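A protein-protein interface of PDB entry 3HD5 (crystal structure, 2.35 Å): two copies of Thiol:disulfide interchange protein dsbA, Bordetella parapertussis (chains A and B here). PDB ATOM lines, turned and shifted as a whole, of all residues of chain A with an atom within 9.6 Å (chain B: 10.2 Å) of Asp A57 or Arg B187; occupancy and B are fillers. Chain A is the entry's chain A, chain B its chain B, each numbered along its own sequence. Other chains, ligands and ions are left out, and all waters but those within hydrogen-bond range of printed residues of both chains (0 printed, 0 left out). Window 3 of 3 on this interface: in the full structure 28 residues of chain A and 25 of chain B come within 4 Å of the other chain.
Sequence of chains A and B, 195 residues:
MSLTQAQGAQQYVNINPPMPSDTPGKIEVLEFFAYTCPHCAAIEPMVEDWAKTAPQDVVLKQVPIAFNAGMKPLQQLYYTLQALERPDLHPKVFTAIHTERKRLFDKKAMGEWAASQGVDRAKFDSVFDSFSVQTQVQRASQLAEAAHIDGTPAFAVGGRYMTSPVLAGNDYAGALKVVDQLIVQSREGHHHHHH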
ATOM      1  N   SER A  21     -13.504  19.371   5.277  1.00  0.00           N
ATOM      2  CA  SER A  21     -13.206  18.135   4.562  1.00  0.00           C
ATOM      3  C   SER A  21     -13.035  16.941   5.497  1.00  0.00           C
ATOM      4  O   SER A  21     -12.421  17.056   6.560  1.00  0.00           O
ATOM      5  CB  SER A  21     -11.938  18.303   3.735  1.00  0.00           C
ATOM      6  OG  SER A  21     -11.563  17.064   3.172  1.00  0.00           O
ATOM      7  N   THR A  23     -11.485  14.262   4.570  1.00  0.00           N
ATOM      8  CA  THR A  23     -10.326  13.550   4.066  1.00  0.00           C
ATOM      9  C   THR A  23      -9.158  14.497   4.298  1.00  0.00           C
ATOM     10  O   THR A  23      -8.934  15.426   3.521  1.00  0.00           O
ATOM     11  CB  THR A  23     -10.457  13.235   2.555  1.00  0.00           C
ATOM     12  OG1 THR A  23     -11.675  12.519   2.320  1.00  0.00           O
ATOM     13  CG2 THR A  23      -9.296  12.377   2.087  1.00  0.00           C
ATOM     14  N   PRO A  24      -8.409  14.279   5.391  1.00  0.00           N
ATOM     15  CA  PRO A  24      -7.262  15.121   5.732  1.00  0.00           C
ATOM     16  C   PRO A  24      -6.334  15.393   4.561  1.00  0.00           C
ATOM     17  O   PRO A  24      -5.921  14.476   3.846  1.00  0.00           O
ATOM     18  CB  PRO A  24      -6.587  14.351   6.872  1.00  0.00           C
ATOM     19  CG  PRO A  24      -7.108  12.935   6.736  1.00  0.00           C
ATOM     20  CD  PRO A  24      -8.533  13.152   6.334  1.00  0.00           C
ATOM     21  N   GLY A  25      -6.039  16.674   4.356  1.00  0.00           N
ATOM     22  CA  GLY A  25      -5.158  17.081   3.276  1.00  0.00           C
ATOM     23  C   GLY A  25      -5.802  17.140   1.906  1.00  0.00           C
ATOM     24  O   GLY A  25      -5.154  17.548   0.938  1.00  0.00           O
ATOM     25  N   LYS A  26      -7.072  16.756   1.812  1.00  0.00           N
ATOM     26  CA  LYS A  26      -7.761  16.762   0.521  1.00  0.00           C
ATOM     27  C   LYS A  26      -8.938  17.721   0.416  1.00  0.00           C
ATOM     28  O   LYS A  26      -9.727  17.858   1.352  1.00  0.00           O
ATOM     29  CB  LYS A  26      -8.292  15.365   0.190  1.00  0.00           C
ATOM     30  CG  LYS A  26      -7.273  14.257   0.232  1.00  0.00           C
ATOM     31  CD  LYS A  26      -6.274  14.373  -0.894  1.00  0.00           C
ATOM     32  CE  LYS A  26      -5.399  13.136  -0.945  1.00  0.00           C
ATOM     33  NZ  LYS A  26      -4.412  13.225  -2.045  1.00  0.00           N
ATOM     34  N   ILE A  27      -9.053  18.376  -0.732  1.00  0.00           N
ATOM     35  CA  ILE A  27     -10.188  19.249  -0.990  1.00  0.00           C
ATOM     36  C   ILE A  27     -11.233  18.256  -1.479  1.00  0.00           C
ATOM     37  O   ILE A  27     -10.989  17.524  -2.443  1.00  0.00           O
ATOM     38  CB  ILE A  27      -9.922  20.214  -2.139  1.00  0.00           C
ATOM     39  CG1 ILE A  27      -8.860  21.237  -1.734  1.00  0.00           C
ATOM     40  CG2 ILE A  27     -11.214  20.888  -2.542  1.00  0.00           C
ATOM     41  CD1 ILE A  27      -8.310  22.029  -2.907  1.00  0.00           C
ATOM     42  N   GLU A  28     -12.387  18.224  -0.823  1.00  0.00           N
ATOM     43  CA  GLU A  28     -13.444  17.299  -1.200  1.00  0.00           C
ATOM     44  C   GLU A  28     -14.462  17.834  -2.189  1.00  0.00           C
ATOM     45  O   GLU A  28     -14.904  18.978  -2.098  1.00  0.00           O
ATOM     46  CB  GLU A  28     -14.220  16.831   0.033  1.00  0.00           C
ATOM     47  CG  GLU A  28     -13.460  15.940   0.989  1.00  0.00           C
ATOM     48  CD  GLU A  28     -14.374  15.327   2.038  1.00  0.00           C
ATOM     49  OE1 GLU A  28     -15.296  16.041   2.500  1.00  0.00           O
ATOM     50  OE2 GLU A  28     -14.170  14.144   2.403  1.00  0.00           O
ATOM     51  N   VAL A  29     -14.832  16.983  -3.138  1.00  0.00           N
ATOM     52  CA  VAL A  29     -15.871  17.309  -4.102  1.00  0.00           C
ATOM     53  C   VAL A  29     -16.908  16.236  -3.838  1.00  0.00           C
ATOM     54  O   VAL A  29     -16.651  15.047  -4.045  1.00  0.00           O
ATOM     55  CB  VAL A  29     -15.413  17.191  -5.565  1.00  0.00           C
ATOM     56  CG1 VAL A  29     -16.628  17.335  -6.484  1.00  0.00           C
ATOM     57  CG2 VAL A  29     -14.392  18.263  -5.886  1.00  0.00           C
ATOM     58  N   TRP A  50     -14.221  12.205 -15.354  1.00  0.00           N
ATOM     59  CA  TRP A  50     -13.709  13.447 -14.797  1.00  0.00           C
ATOM     60  C   TRP A  50     -12.771  13.175 -13.625  1.00  0.00           C
ATOM     61  O   TRP A  50     -11.715  13.789 -13.513  1.00  0.00           O
ATOM     62  CB  TRP A  50     -14.865  14.324 -14.308  1.00  0.00           C
ATOM     63  CG  TRP A  50     -14.402  15.556 -13.578  1.00  0.00           C
ATOM     64  CD1 TRP A  50     -14.016  16.735 -14.136  1.00  0.00           C
ATOM     65  CD2 TRP A  50     -14.219  15.703 -12.162  1.00  0.00           C
ATOM     66  NE1 TRP A  50     -13.600  17.611 -13.162  1.00  0.00           N
ATOM     67  CE2 TRP A  50     -13.712  17.002 -11.939  1.00  0.00           C
ATOM     68  CE3 TRP A  50     -14.432  14.859 -11.059  1.00  0.00           C
ATOM     69  CZ2 TRP A  50     -13.409  17.484 -10.657  1.00  0.00           C
ATOM     70  CZ3 TRP A  50     -14.131  15.338  -9.781  1.00  0.00           C
ATOM     71  CH2 TRP A  50     -13.623  16.644  -9.595  1.00  0.00           C
ATOM     72  N   THR A  53      -8.908  12.338 -14.019  1.00  0.00           N
ATOM     73  CA  THR A  53      -7.933  13.394 -14.260  1.00  0.00           C
ATOM     74  C   THR A  53      -8.046  14.539 -13.264  1.00  0.00           C
ATOM     75  O   THR A  53      -7.494  15.617 -13.485  1.00  0.00           O
ATOM     76  CB  THR A  53      -8.085  13.984 -15.674  1.00  0.00           C
ATOM     77  OG1 THR A  53      -9.411  14.507 -15.829  1.00  0.00           O
ATOM     78  CG2 THR A  53      -7.837  12.924 -16.726  1.00  0.00           C
ATOM     79  N   ALA A  54      -8.760  14.310 -12.169  1.00  0.00           N
ATOM     80  CA  ALA A  54      -8.940  15.339 -11.159  1.00  0.00           C
ATOM     81  C   ALA A  54      -7.624  15.692 -10.470  1.00  0.00           C
ATOM     82  O   ALA A  54      -6.677  14.908 -10.486  1.00  0.00           O
ATOM     83  CB  ALA A  54      -9.959  14.885 -10.136  1.00  0.00           C
ATOM     84  N   PRO A  55      -7.548  16.893  -9.868  1.00  0.00           N
ATOM     85  CA  PRO A  55      -6.345  17.358  -9.165  1.00  0.00           C
ATOM     86  C   PRO A  55      -5.926  16.416  -8.032  1.00  0.00           C
ATOM     87  O   PRO A  55      -6.769  15.880  -7.303  1.00  0.00           O
ATOM     88  CB  PRO A  55      -6.759  18.737  -8.657  1.00  0.00           C
ATOM     89  CG  PRO A  55      -7.714  19.205  -9.709  1.00  0.00           C
ATOM     90  CD  PRO A  55      -8.551  17.971  -9.947  1.00  0.00           C
ATOM     91  N   GLN A  56      -4.621  16.226  -7.884  1.00  0.00           N
ATOM     92  CA  GLN A  56      -4.086  15.328  -6.866  1.00  0.00           C
ATOM     93  C   GLN A  56      -4.496  15.638  -5.428  1.00  0.00           C
ATOM     94  O   GLN A  56      -4.590  14.736  -4.592  1.00  0.00           O
ATOM     95  CB  GLN A  56      -2.561  15.283  -6.976  1.00  0.00           C
ATOM     96  CG  GLN A  56      -2.073  14.787  -8.334  1.00  0.00           C
ATOM     97  CD  GLN A  56      -2.744  13.480  -8.762  1.00  0.00           C
ATOM     98  OE1 GLN A  56      -2.572  12.435  -8.121  1.00  0.00           O
ATOM     99  NE2 GLN A  56      -3.519  13.538  -9.847  1.00  0.00           N
ATOM    100  N   ASP A  57      -4.749  16.907  -5.144  1.00  0.00           N
ATOM    101  CA  ASP A  57      -5.139  17.322  -3.803  1.00  0.00           C
ATOM    102  C   ASP A  57      -6.660  17.329  -3.669  1.00  0.00           C
ATOM    103  O   ASP A  57      -7.212  17.848  -2.691  1.00  0.00           O
ATOM    104  CB  ASP A  57      -4.582  18.713  -3.526  1.00  0.00           C
ATOM    105  CG  ASP A  57      -5.038  19.730  -4.550  1.00  0.00           C
ATOM    106  OD1 ASP A  57      -5.296  19.328  -5.704  1.00  0.00           O
ATOM    107  OD2 ASP A  57      -5.124  20.929  -4.210  1.00  0.00           O
ATOM    108  N   VAL A  58      -7.327  16.736  -4.656  1.00  0.00           N
ATOM    109  CA  VAL A  58      -8.781  16.681  -4.678  1.00  0.00           C
ATOM    110  C   VAL A  58      -9.280  15.251  -4.631  1.00  0.00           C
ATOM    111  O   VAL A  58      -8.701  14.363  -5.240  1.00  0.00           O
ATOM    112  CB  VAL A  58      -9.348  17.338  -5.962  1.00  0.00           C
ATOM    113  CG1 VAL A  58     -10.846  17.083  -6.061  1.00  0.00           C
ATOM    114  CG2 VAL A  58      -9.073  18.825  -5.948  1.00  0.00           C
ATOM    115  N   VAL A  59     -10.361  15.026  -3.904  1.00  0.00           N
ATOM    116  CA  VAL A  59     -10.917  13.691  -3.846  1.00  0.00           C
ATOM    117  C   VAL A  59     -12.405  13.801  -4.129  1.00  0.00           C
ATOM    118  O   VAL A  59     -13.063  14.747  -3.693  1.00  0.00           O
ATOM    119  CB  VAL A  59     -10.673  13.025  -2.464  1.00  0.00           C
ATOM    120  CG1 VAL A  59     -11.872  13.202  -1.550  1.00  0.00           C
ATOM    121  CG2 VAL A  59     -10.367  11.559  -2.653  1.00  0.00           C
ATOM    122  N   LEU A  60     -12.931  12.847  -4.882  1.00  0.00           N
ATOM    123  CA  LEU A  60     -14.347  12.850  -5.206  1.00  0.00           C
ATOM    124  C   LEU A  60     -15.086  11.809  -4.383  1.00  0.00           C
ATOM    125  O   LEU A  60     -14.625  10.685  -4.233  1.00  0.00           O
ATOM    126  CB  LEU A  60     -14.560  12.551  -6.688  1.00  0.00           C
ATOM    127  CG  LEU A  60     -16.037  12.343  -7.036  1.00  0.00           C
ATOM    128  CD1 LEU A  60     -16.763  13.694  -7.035  1.00  0.00           C
ATOM    129  CD2 LEU A  60     -16.152  11.673  -8.387  1.00  0.00           C
ATOM    130  N   VAL A 157     -18.294  21.710  -3.279  1.00  0.00           N
ATOM    131  CA  VAL A 157     -16.862  21.811  -3.518  1.00  0.00           C
ATOM    132  C   VAL A 157     -16.136  22.532  -2.390  1.00  0.00           C
ATOM    133  O   VAL A 157     -16.516  23.639  -1.988  1.00  0.00           O
ATOM    134  CB  VAL A 157     -16.585  22.556  -4.833  1.00  0.00           C
ATOM    135  CG1 VAL A 157     -15.098  22.615  -5.082  1.00  0.00           C
ATOM    136  CG2 VAL A 157     -17.298  21.857  -5.996  1.00  0.00           C
ATOM    137  N   GLY A 158     -15.085  21.891  -1.887  1.00  0.00           N
ATOM    138  CA  GLY A 158     -14.300  22.463  -0.810  1.00  0.00           C
ATOM    139  C   GLY A 158     -15.144  22.854   0.388  1.00  0.00           C
ATOM    140  O   GLY A 158     -14.739  23.702   1.178  1.00  0.00           O
ATOM    141  N   GLY A 159     -16.315  22.237   0.517  1.00  0.00           N
ATOM    142  CA  GLY A 159     -17.211  22.535   1.621  1.00  0.00           C
ATOM    143  C   GLY A 159     -17.771  23.949   1.595  1.00  0.00           C
ATOM    144  O   GLY A 159     -18.580  24.309   2.446  1.00  0.00           O
ATOM    145  N   ARG A 160     -17.355  24.736   0.606  1.00  0.00           N
ATOM    146  CA  ARG A 160     -17.778  26.132   0.467  1.00  0.00           C
ATOM    147  C   ARG A 160     -18.843  26.412  -0.591  1.00  0.00           C
ATOM    148  O   ARG A 160     -19.653  27.331  -0.438  1.00  0.00           O
ATOM    149  CB  ARG A 160     -16.574  27.013   0.127  1.00  0.00           C
ATOM    150  CG  ARG A 160     -15.587  27.288   1.249  1.00  0.00           C
ATOM    151  CD  ARG A 160     -14.474  28.164   0.687  1.00  0.00           C
ATOM    152  NE  ARG A 160     -13.476  28.567   1.672  1.00  0.00           N
ATOM    153  CZ  ARG A 160     -12.454  29.377   1.397  1.00  0.00           C
ATOM    154  NH1 ARG A 160     -12.305  29.861   0.168  1.00  0.00           N
ATOM    155  NH2 ARG A 160     -11.590  29.717   2.349  1.00  0.00           N
ATOM    156  N   TYR A 161     -18.834  25.637  -1.670  1.00  0.00           N
ATOM    157  CA  TYR A 161     -19.784  25.870  -2.752  1.00  0.00           C
ATOM    158  C   TYR A 161     -20.651  24.693  -3.174  1.00  0.00           C
ATOM    159  O   TYR A 161     -20.283  23.521  -3.046  1.00  0.00           O
ATOM    160  CB  TYR A 161     -19.032  26.389  -3.977  1.00  0.00           C
ATOM    161  CG  TYR A 161     -17.954  27.375  -3.624  1.00  0.00           C
ATOM    162  CD1 TYR A 161     -18.261  28.558  -2.959  1.00  0.00           C
ATOM    163  CD2 TYR A 161     -16.619  27.115  -3.929  1.00  0.00           C
ATOM    164  CE1 TYR A 161     -17.267  29.462  -2.605  1.00  0.00           C
ATOM    165  CE2 TYR A 161     -15.615  28.013  -3.580  1.00  0.00           C
ATOM    166  CZ  TYR A 161     -15.947  29.186  -2.916  1.00  0.00           C
ATOM    167  OH  TYR A 161     -14.963  30.081  -2.552  1.00  0.00           O
ATOM    168  N   VAL B 179     -17.263  23.148 -11.535  1.00  0.00           N
ATOM    169  CA  VAL B 179     -16.645  22.416 -10.434  1.00  0.00           C
ATOM    170  C   VAL B 179     -15.129  22.624 -10.450  1.00  0.00           C
ATOM    171  O   VAL B 179     -14.520  22.829  -9.399  1.00  0.00           O
ATOM    172  CB  VAL B 179     -16.959  20.888 -10.512  1.00  0.00           C
ATOM    173  CG1 VAL B 179     -16.101  20.123  -9.516  1.00  0.00           C
ATOM    174  CG2 VAL B 179     -18.425  20.639 -10.210  1.00  0.00           C
ATOM    175  N   ASP B 180     -14.521  22.576 -11.634  1.00  0.00           N
ATOM    176  CA  ASP B 180     -13.077  22.766 -11.732  1.00  0.00           C
ATOM    177  C   ASP B 180     -12.681  24.135 -11.194  1.00  0.00           C
ATOM    178  O   ASP B 180     -11.778  24.256 -10.360  1.00  0.00           O
ATOM    179  CB  ASP B 180     -12.597  22.635 -13.182  1.00  0.00           C
ATOM    180  CG  ASP B 180     -12.703  21.211 -13.709  1.00  0.00           C
ATOM    181  OD1 ASP B 180     -12.642  20.271 -12.891  1.00  0.00           O
ATOM    182  OD2 ASP B 180     -12.834  21.028 -14.939  1.00  0.00           O
ATOM    183  N   GLN B 181     -13.378  25.161 -11.669  1.00  0.00           N
ATOM    184  CA  GLN B 181     -13.115  26.531 -11.260  1.00  0.00           C
ATOM    185  C   GLN B 181     -13.373  26.718  -9.766  1.00  0.00           C
ATOM    186  O   GLN B 181     -12.672  27.484  -9.104  1.00  0.00           O
ATOM    187  CB  GLN B 181     -13.976  27.489 -12.093  1.00  0.00           C
ATOM    188  CG  GLN B 181     -13.699  27.373 -13.603  1.00  0.00           C
ATOM    189  CD  GLN B 181     -14.713  28.108 -14.477  1.00  0.00           C
ATOM    190  OE1 GLN B 181     -15.920  27.879 -14.380  1.00  0.00           O
ATOM    191  NE2 GLN B 181     -14.220  28.986 -15.346  1.00  0.00           N
ATOM    192  N   LEU B 182     -14.374  26.021  -9.235  1.00  0.00           N
ATOM    193  CA  LEU B 182     -14.678  26.122  -7.816  1.00  0.00           C
ATOM    194  C   LEU B 182     -13.568  25.462  -6.992  1.00  0.00           C
ATOM    195  O   LEU B 182     -13.298  25.872  -5.860  1.00  0.00           O
ATOM    196  CB  LEU B 182     -16.033  25.479  -7.507  1.00  0.00           C
ATOM    197  CG  LEU B 182     -17.260  26.284  -7.958  1.00  0.00           C
ATOM    198  CD1 LEU B 182     -18.537  25.584  -7.518  1.00  0.00           C
ATOM    199  CD2 LEU B 182     -17.206  27.686  -7.356  1.00  0.00           C
ATOM    200  N   ILE B 183     -12.928  24.441  -7.561  1.00  0.00           N
ATOM    201  CA  ILE B 183     -11.829  23.755  -6.884  1.00  0.00           C
ATOM    202  C   ILE B 183     -10.686  24.759  -6.734  1.00  0.00           C
ATOM    203  O   ILE B 183     -10.044  24.858  -5.685  1.00  0.00           O
ATOM    204  CB  ILE B 183     -11.337  22.528  -7.702  1.00  0.00           C
ATOM    205  CG1 ILE B 183     -12.321  21.367  -7.535  1.00  0.00           C
ATOM    206  CG2 ILE B 183      -9.948  22.103  -7.253  1.00  0.00           C
ATOM    207  CD1 ILE B 183     -12.028  20.188  -8.441  1.00  0.00           C
ATOM    208  N   VAL B 184     -10.437  25.507  -7.799  1.00  0.00           N
ATOM    209  CA  VAL B 184      -9.385  26.506  -7.779  1.00  0.00           C
ATOM    210  C   VAL B 184      -9.736  27.583  -6.762  1.00  0.00           C
ATOM    211  O   VAL B 184      -8.913  27.971  -5.940  1.00  0.00           O
ATOM    212  CB  VAL B 184      -9.222  27.154  -9.161  1.00  0.00           C
ATOM    213  CG1 VAL B 184      -8.167  28.247  -9.101  1.00  0.00           C
ATOM    214  CG2 VAL B 184      -8.842  26.094 -10.180  1.00  0.00           C
ATOM    215  N   GLN B 185     -10.975  28.044  -6.814  1.00  0.00           N
ATOM    216  CA  GLN B 185     -11.444  29.093  -5.921  1.00  0.00           C
ATOM    217  C   GLN B 185     -11.228  28.789  -4.441  1.00  0.00           C
ATOM    218  O   GLN B 185     -10.792  29.655  -3.680  1.00  0.00           O
ATOM    219  CB  GLN B 185     -12.924  29.362  -6.186  1.00  0.00           C
ATOM    220  CG  GLN B 185     -13.406  30.689  -5.669  1.00  0.00           C
ATOM    221  CD  GLN B 185     -14.662  31.138  -6.365  1.00  0.00           C
ATOM    222  OE1 GLN B 185     -14.709  31.202  -7.594  1.00  0.00           O
ATOM    223  NE2 GLN B 185     -15.693  31.457  -5.588  1.00  0.00           N
ATOM    224  N   SER B 186     -11.533  27.562  -4.037  1.00  0.00           N
ATOM    225  CA  SER B 186     -11.381  27.151  -2.647  1.00  0.00           C
ATOM    226  C   SER B 186      -9.917  26.972  -2.244  1.00  0.00           C
ATOM    227  O   SER B 186      -9.504  27.408  -1.169  1.00  0.00           O
ATOM    228  CB  SER B 186     -12.131  25.842  -2.411  1.00  0.00           C
ATOM    229  OG  SER B 186     -11.580  24.818  -3.216  1.00  0.00           O
ATOM    230  N   ARG B 187      -9.142  26.323  -3.103  1.00  0.00           N
ATOM    231  CA  ARG B 187      -7.730  26.083  -2.836  1.00  0.00           C
ATOM    232  C   ARG B 187      -6.997  27.393  -2.556  1.00  0.00           C
ATOM    233  O   ARG B 187      -5.871  27.382  -2.063  1.00  0.00           O
ATOM    234  CB  ARG B 187      -7.106  25.353  -4.029  1.00  0.00           C
ATOM    235  CG  ARG B 187      -5.637  24.964  -3.886  1.00  0.00           C
ATOM    236  CD  ARG B 187      -5.327  23.742  -4.755  1.00  0.00           C
ATOM    237  NE  ARG B 187      -5.870  23.887  -6.104  1.00  0.00           N
ATOM    238  CZ  ARG B 187      -6.231  22.872  -6.885  1.00  0.00           C
ATOM    239  NH1 ARG B 187      -6.106  21.626  -6.453  1.00  0.00           N
ATOM    240  NH2 ARG B 187      -6.732  23.102  -8.094  1.00  0.00           N
ATOM    241  N   GLU B 188      -7.649  28.515  -2.863  1.00  0.00           N
ATOM    242  CA  GLU B 188      -7.071  29.844  -2.647  1.00  0.00           C
ATOM    243  C   GLU B 188      -7.445  30.409  -1.281  1.00  0.00           C
ATOM    244  O   GLU B 188      -7.938  29.640  -0.424  1.00  0.00           O
ATOM    245  CB  GLU B 188      -7.537  30.830  -3.727  1.00  0.00           C
ATOM    246  CG  GLU B 188      -7.338  30.361  -5.158  1.00  0.00           C
ATOM    247  CD  GLU B 188      -5.972  29.744  -5.399  1.00  0.00           C
ATOM    248  OE1 GLU B 188      -5.693  28.667  -4.824  1.00  0.00           O
ATOM    249  OE2 GLU B 188      -5.176  30.336  -6.162  1.00  0.00           O
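The indole nitrogen (NE1) of Trp A50 is in hydrogen-bond range of the side-chain carboxylate (OD1) of Asp B180 (2.8 Å). The guanidinium group (NH1) of Arg B187 lies within salt-bridge range of the side-chain carboxylate (OD2) of Asp A57 (2.5 Å). The side-chain hydroxyl of Tyr A161 lies within hydrogen-bond range of the side-chain amide nitrogen of Gln B185 (3.4 Å).
O of Asp A57 lies within hydrogen-bond range of N of Ile A27 (2.7 Å). The backbone carbonyl oxygen (O) of Trp A50 lies within hydrogen-bond range of the side-chain hydroxyl (OG1) of Thr A53, 3.3 Å away. O of Ile A27 is in hydrogen-bond range of N of Val A59. The backbone carbonyl oxygen (O) of Ile B183 is in hydrogen-bond range of the side-chain hydroxyl (OG) of Ser B186 (2.9 Å). The backbone NH (N) of Val A29 sits at hydrogen-bond distance from the backbone carbonyl oxygen (O) of Val A59. O of Leu B182 is in hydrogen-bond range of OG of Ser B186 (3.3 Å).
Arg B187 touches Ile A27 (CB to CD1, 3.7 Å). Val A29 touches Ile B183. CG1 of Val B179 touches CZ2 of Trp A50, 3.9 Å away. CZ2 of Trp A50 touches CD1 of Ile B183, at 3.8 Å. Pro A55 touches Arg B187. Ile B183 touches Val A58. CG1 of Val A157 touches C of Leu B182, 3.8 Å away. Val A157 touches Ile B183 (CG1 to N, 3.8 Å). Ser B186 touches Arg A160. Tyr A161 touches Leu B182 (CD2 to CD2, 3.5 Å).
Of chain B, only Arg B187 comes within 4 Å of Asp A57. Of chain A, only Ile A27 (3.7 Å), Pro A55 (3.7 Å) and Asp A57 (2.5 Å) come within 4 Å of Arg B187. Lys A26 touches none of the printed residues of chain B. Pro A55 touches one residue of chain B. Of chain B, only Ile B183 (3.6 Å) comes within 4 Å of Val A58. No residue of chain A comes within 4 Å of Val B184. No residue of chain A comes within 4 Å of Glu B188. Printed residues of chain A within 4 Å of Gln B185: Tyr A161. Printed residues of chain B within 4 Å of Tyr A161: Leu B182 and Gln B185. Printed residues of chain B within 4 Å of Val A157: Leu B182 and Ile B183. Ser A21 touches none of the printed residues of chain B. Val A59 touches none of the printed residues of chain B. The nearest residue of chain B that does not touch Asp A57 is Ile B183 (5.6 Å).
Of the 22 printed residues of chain A, 9 touch a printed residue of chain B. Printed residues of chain B that touch a printed residue of chain A: Val B179, Asp B180, Leu B182, Ile B183, Gln B185, Ser B186 and Arg B187. Hydrophobic or aromatic side chains of chain B within 4 Å of the printed part of chain A: Val B179, Leu B182 and Ile B183. Among the printed residues, Asp or Glu carboxylates within 4 Å of a Lys or Arg side-chain nitrogen of the other chain: Asp A57 with Arg B187 (2.5 Å).
No position is printed for both chains. Of the 13 pairs that touch across the chains among the printed residues, none has its exchanged pair printed and touching as well.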
